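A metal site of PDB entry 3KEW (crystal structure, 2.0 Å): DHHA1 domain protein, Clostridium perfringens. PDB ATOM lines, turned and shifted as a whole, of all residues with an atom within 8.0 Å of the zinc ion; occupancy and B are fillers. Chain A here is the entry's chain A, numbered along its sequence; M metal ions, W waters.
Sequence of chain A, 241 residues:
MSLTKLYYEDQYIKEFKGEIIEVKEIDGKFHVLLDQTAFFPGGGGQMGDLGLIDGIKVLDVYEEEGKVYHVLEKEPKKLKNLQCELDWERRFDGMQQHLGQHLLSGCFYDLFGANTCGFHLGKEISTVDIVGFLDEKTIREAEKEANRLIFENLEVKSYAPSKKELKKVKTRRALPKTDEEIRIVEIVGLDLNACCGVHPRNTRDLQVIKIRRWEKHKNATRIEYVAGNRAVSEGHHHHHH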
ATOM      1  N   GLY A  43      17.725 -22.449  -1.245  1.00  0.00           N
ATOM      2  CA  GLY A  43      18.733 -23.483  -1.472  1.00  0.00           C
ATOM      3  C   GLY A  43      18.519 -24.753  -0.663  1.00  0.00           C
ATOM      4  O   GLY A  43      18.054 -24.710   0.470  1.00  0.00           O
ATOM      5  N   GLY A  44      18.835 -25.895  -1.260  1.00  0.00           N
ATOM      6  CA  GLY A  44      18.642 -27.208  -0.628  1.00  0.00           C
ATOM      7  C   GLY A  44      17.206 -27.582  -0.252  1.00  0.00           C
ATOM      8  O   GLY A  44      16.996 -28.439   0.615  1.00  0.00           O
ATOM      9  N   GLY A  45      16.233 -26.946  -0.897  1.00  0.00           N
ATOM     10  CA  GLY A  45      14.819 -27.168  -0.590  1.00  0.00           C
ATOM     11  C   GLY A  45      14.203 -26.085   0.281  1.00  0.00           C
ATOM     12  O   GLY A  45      12.975 -26.031   0.448  1.00  0.00           O
ATOM     13  N   GLN A  46      15.046 -25.224   0.837  1.00  0.00           N
ATOM     14  CA  GLN A  46      14.623 -24.217   1.781  1.00  0.00           C
ATOM     15  C   GLN A  46      14.312 -22.925   1.049  1.00  0.00           C
ATOM     16  O   GLN A  46      15.054 -22.524   0.150  1.00  0.00           O
ATOM     17  CB  GLN A  46      15.740 -24.005   2.797  1.00  0.00           C
ATOM     18  CG  GLN A  46      15.472 -23.011   3.916  1.00  0.00           C
ATOM     19  CD  GLN A  46      16.560 -23.081   4.947  1.00  0.00           C
ATOM     20  OE1 GLN A  46      17.451 -23.956   4.872  1.00  0.00           O
ATOM     21  NE2 GLN A  46      16.540 -22.158   5.917  1.00  0.00           N
ATOM     22  N   HIS A  98      14.118 -27.435   8.317  1.00  0.00           N
ATOM     23  CA  HIS A  98      15.194 -28.076   7.571  1.00  0.00           C
ATOM     24  C   HIS A  98      16.066 -28.944   8.480  1.00  0.00           C
ATOM     25  O   HIS A  98      16.352 -30.092   8.151  1.00  0.00           O
ATOM     26  CB  HIS A  98      16.046 -27.024   6.842  1.00  0.00           C
ATOM     27  CG  HIS A  98      16.854 -27.570   5.696  1.00  0.00           C
ATOM     28  ND1 HIS A  98      17.279 -26.783   4.662  1.00  0.00           N
ATOM     29  CD2 HIS A  98      17.301 -28.821   5.430  1.00  0.00           C
ATOM     30  CE1 HIS A  98      17.967 -27.507   3.808  1.00  0.00           C
ATOM     31  NE2 HIS A  98      17.996 -28.752   4.243  1.00  0.00           N
ATOM     32  N   LEU A  99      16.512 -28.384   9.607  1.00  0.00           N
ATOM     33  CA  LEU A  99      17.288 -29.161  10.574  1.00  0.00           C
ATOM     34  C   LEU A  99      16.415 -30.292  11.151  1.00  0.00           C
ATOM     35  O   LEU A  99      16.917 -31.392  11.382  1.00  0.00           O
ATOM     36  CB  LEU A  99      17.871 -28.270  11.697  1.00  0.00           C
ATOM     37  CG  LEU A  99      18.591 -28.965  12.872  1.00  0.00           C
ATOM     38  CD1 LEU A  99      19.774 -29.785  12.401  1.00  0.00           C
ATOM     39  CD2 LEU A  99      19.036 -27.995  13.958  1.00  0.00           C
ATOM     40  N   GLN A 101      14.155 -32.048   9.570  1.00  0.00           N
ATOM     41  CA  GLN A 101      14.319 -33.128   8.592  1.00  0.00           C
ATOM     42  C   GLN A 101      15.640 -33.879   8.750  1.00  0.00           C
ATOM     43  O   GLN A 101      15.633 -35.111   8.789  1.00  0.00           O
ATOM     44  CB  GLN A 101      14.179 -32.616   7.167  1.00  0.00           C
ATOM     45  CG  GLN A 101      14.375 -33.690   6.088  1.00  0.00           C
ATOM     46  CD  GLN A 101      15.747 -33.626   5.477  1.00  0.00           C
ATOM     47  OE1 GLN A 101      16.133 -32.580   4.960  1.00  0.00           O
ATOM     48  NE2 GLN A 101      16.507 -34.729   5.543  1.00  0.00           N
ATOM     49  N   HIS A 102      16.748 -33.149   8.815  1.00  0.00           N
ATOM     50  CA  HIS A 102      18.084 -33.762   8.992  1.00  0.00           C
ATOM     51  C   HIS A 102      18.172 -34.617  10.256  1.00  0.00           C
ATOM     52  O   HIS A 102      18.786 -35.692  10.262  1.00  0.00           O
ATOM     53  CB  HIS A 102      19.170 -32.682   9.078  1.00  0.00           C
ATOM     54  CG  HIS A 102      19.608 -32.126   7.755  1.00  0.00           C
ATOM     55  ND1 HIS A 102      20.933 -32.050   7.389  1.00  0.00           N
ATOM     56  CD2 HIS A 102      18.901 -31.601   6.731  1.00  0.00           C
ATOM     57  CE1 HIS A 102      21.025 -31.514   6.194  1.00  0.00           C
ATOM     58  NE2 HIS A 102      19.809 -31.227   5.772  1.00  0.00           N
ATOM     59  N   PHE A 119      12.631 -35.424   0.550  1.00  0.00           N
ATOM     60  CA  PHE A 119      12.174 -34.448   1.551  1.00  0.00           C
ATOM     61  C   PHE A 119      11.474 -33.285   0.849  1.00  0.00           C
ATOM     62  O   PHE A 119      11.755 -32.989  -0.302  1.00  0.00           O
ATOM     63  CB  PHE A 119      13.312 -33.928   2.458  1.00  0.00           C
ATOM     64  CG  PHE A 119      14.592 -33.594   1.729  1.00  0.00           C
ATOM     65  CD1 PHE A 119      14.800 -32.326   1.204  1.00  0.00           C
ATOM     66  CD2 PHE A 119      15.609 -34.546   1.591  1.00  0.00           C
ATOM     67  CE1 PHE A 119      15.980 -32.005   0.523  1.00  0.00           C
ATOM     68  CE2 PHE A 119      16.796 -34.243   0.922  1.00  0.00           C
ATOM     69  CZ  PHE A 119      16.982 -32.972   0.388  1.00  0.00           C
ATOM     70  N   LEU A 121      10.091 -29.259   2.029  1.00  0.00           N
ATOM     71  CA  LEU A 121       9.839 -28.224   3.024  1.00  0.00           C
ATOM     72  C   LEU A 121       8.806 -27.274   2.451  1.00  0.00           C
ATOM     73  O   LEU A 121       9.074 -26.553   1.493  1.00  0.00           O
ATOM     74  CB  LEU A 121      11.139 -27.477   3.372  1.00  0.00           C
ATOM     75  CG  LEU A 121      12.390 -28.322   3.669  1.00  0.00           C
ATOM     76  CD1 LEU A 121      13.602 -27.420   3.781  1.00  0.00           C
ATOM     77  CD2 LEU A 121      12.225 -29.127   4.946  1.00  0.00           C
ATOM     78  N   VAL A 185      26.689 -29.730   6.384  1.00  0.00           N
ATOM     79  CA  VAL A 185      25.963 -29.563   7.643  1.00  0.00           C
ATOM     80  C   VAL A 185      26.105 -30.833   8.464  1.00  0.00           C
ATOM     81  O   VAL A 185      25.719 -31.924   8.031  1.00  0.00           O
ATOM     82  CB  VAL A 185      24.470 -29.247   7.422  1.00  0.00           C
ATOM     83  CG1 VAL A 185      23.732 -29.215   8.760  1.00  0.00           C
ATOM     84  CG2 VAL A 185      24.322 -27.921   6.700  1.00  0.00           C
ATOM     85  N   ASN A 193      26.011 -34.413   6.310  1.00  0.00           N
ATOM     86  CA  ASN A 193      25.510 -34.382   4.879  1.00  0.00           C
ATOM     87  C   ASN A 193      25.889 -33.031   4.145  1.00  0.00           C
ATOM     88  O   ASN A 193      25.893 -31.979   4.717  1.00  0.00           O
ATOM     89  CB  ASN A 193      23.981 -34.532   4.840  1.00  0.00           C
ATOM     90  CG  ASN A 193      23.478 -35.763   5.590  1.00  0.00           C
ATOM     91  OD1 ASN A 193      23.389 -36.853   5.043  1.00  0.00           O
ATOM     92  ND2 ASN A 193      23.115 -35.562   6.847  1.00  0.00           N
ATOM     93  N   ALA A 194      25.996 -33.166   2.840  1.00  0.00           N
ATOM     94  CA  ALA A 194      26.193 -31.983   2.023  1.00  0.00           C
ATOM     95  C   ALA A 194      24.846 -31.290   1.942  1.00  0.00           C
ATOM     96  O   ALA A 194      23.834 -31.921   1.612  1.00  0.00           O
ATOM     97  CB  ALA A 194      26.721 -32.352   0.648  1.00  0.00           C
ATOM     98  N   CYS A 195      24.834 -30.014   2.284  1.00  0.00           N
ATOM     99  CA  CYS A 195      23.602 -29.217   2.312  1.00  0.00           C
ATOM    100  C   CYS A 195      23.898 -27.741   2.119  1.00  0.00           C
ATOM    101  O   CYS A 195      24.811 -27.202   2.735  1.00  0.00           O
ATOM    102  CB  CYS A 195      22.843 -29.422   3.643  1.00  0.00           C
ATOM    103  SG  CYS A 195      21.265 -28.597   3.660  1.00  0.00           S
ATOM    104  N   CYS A 196      23.102 -27.098   1.258  1.00  0.00           N
ATOM    105  CA  CYS A 196      23.166 -25.663   1.002  1.00  0.00           C
ATOM    106  C   CYS A 196      22.167 -24.880   1.863  1.00  0.00           C
ATOM    107  O   CYS A 196      21.943 -23.681   1.640  1.00  0.00           O
ATOM    108  CB  CYS A 196      22.851 -25.377  -0.478  1.00  0.00           C
ATOM    109  SG  CYS A 196      24.070 -26.009  -1.624  1.00  0.00           S
ATOM    110  N   GLY A 197      21.548 -25.561   2.815  1.00  0.00           N
ATOM    111  CA  GLY A 197      20.577 -24.912   3.695  1.00  0.00           C
ATOM    112  C   GLY A 197      21.216 -23.977   4.707  1.00  0.00           C
ATOM    113  O   GLY A 197      22.442 -23.978   4.897  1.00  0.00           O
ATOM    114  N   VAL A 198      20.377 -23.157   5.322  1.00  0.00           N
ATOM    115  CA  VAL A 198      20.736 -22.346   6.484  1.00  0.00           C
ATOM    116  C   VAL A 198      20.097 -22.974   7.734  1.00  0.00           C
ATOM    117  O   VAL A 198      18.868 -22.979   7.882  1.00  0.00           O
ATOM    118  CB  VAL A 198      20.351 -20.850   6.269  1.00  0.00           C
ATOM    119  CG1 VAL A 198      20.383 -20.058   7.581  1.00  0.00           C
ATOM    120  CG2 VAL A 198      21.299 -20.210   5.239  1.00  0.00           C
ATOM    121  N   HIS A 199      20.953 -23.518   8.594  1.00  0.00           N
ATOM    122  CA  HIS A 199      20.533 -24.283   9.764  1.00  0.00           C
ATOM    123  C   HIS A 199      20.792 -23.545  11.084  1.00  0.00           C
ATOM    124  O   HIS A 199      21.682 -22.681  11.154  1.00  0.00           O
ATOM    125  CB  HIS A 199      21.258 -25.635   9.759  1.00  0.00           C
ATOM    126  CG  HIS A 199      20.801 -26.557   8.667  1.00  0.00           C
ATOM    127  ND1 HIS A 199      19.916 -27.579   8.895  1.00  0.00           N
ATOM    128  CD2 HIS A 199      21.081 -26.580   7.348  1.00  0.00           C
ATOM    129  CE1 HIS A 199      19.678 -28.208   7.755  1.00  0.00           C
ATOM    130  NE2 HIS A 199      20.369 -27.620   6.804  1.00  0.00           N
HETATM  131 ZN    ZN M   1      19.475 -30.441   3.638  1.00  0.00          ZN
HETATM  132  O   HOH W   1      18.840 -29.971   1.359  1.00  0.00           O
HETATM  133  O   HOH W   2      20.809 -31.978   2.725  1.00  0.00           O
HETATM  134  O   HOH W   3      18.057 -32.273   3.475  1.00  0.00           O
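The side-chain amide oxygen of Gln 46 lies within hydrogen-bond range of a ring nitrogen (ND1) of His 98 (2.8 Å). The side-chain sulfur (SG) of Cys 195 lies close to the backbone NH (N) of Gly 197, 3.2 Å away. NE2 of His 199 sits close to SG of Cys 195, at 3.4 Å.
Of the 18 residues printed, 3 come within 4 Å of the zinc ion. The nearest printed residue that does not touch the zinc ion is Gln 101 (4.2 Å).
The zinc ion is bound by water W2 (2.2 Å), a ring nitrogen (NE2) of His 102 (2.3 Å), water W3 (2.3 Å), a ring nitrogen (NE2) of His 98 (2.3 Å), water W1 (2.4 Å) and the side-chain sulfur of Cys 195 (2.6 Å).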
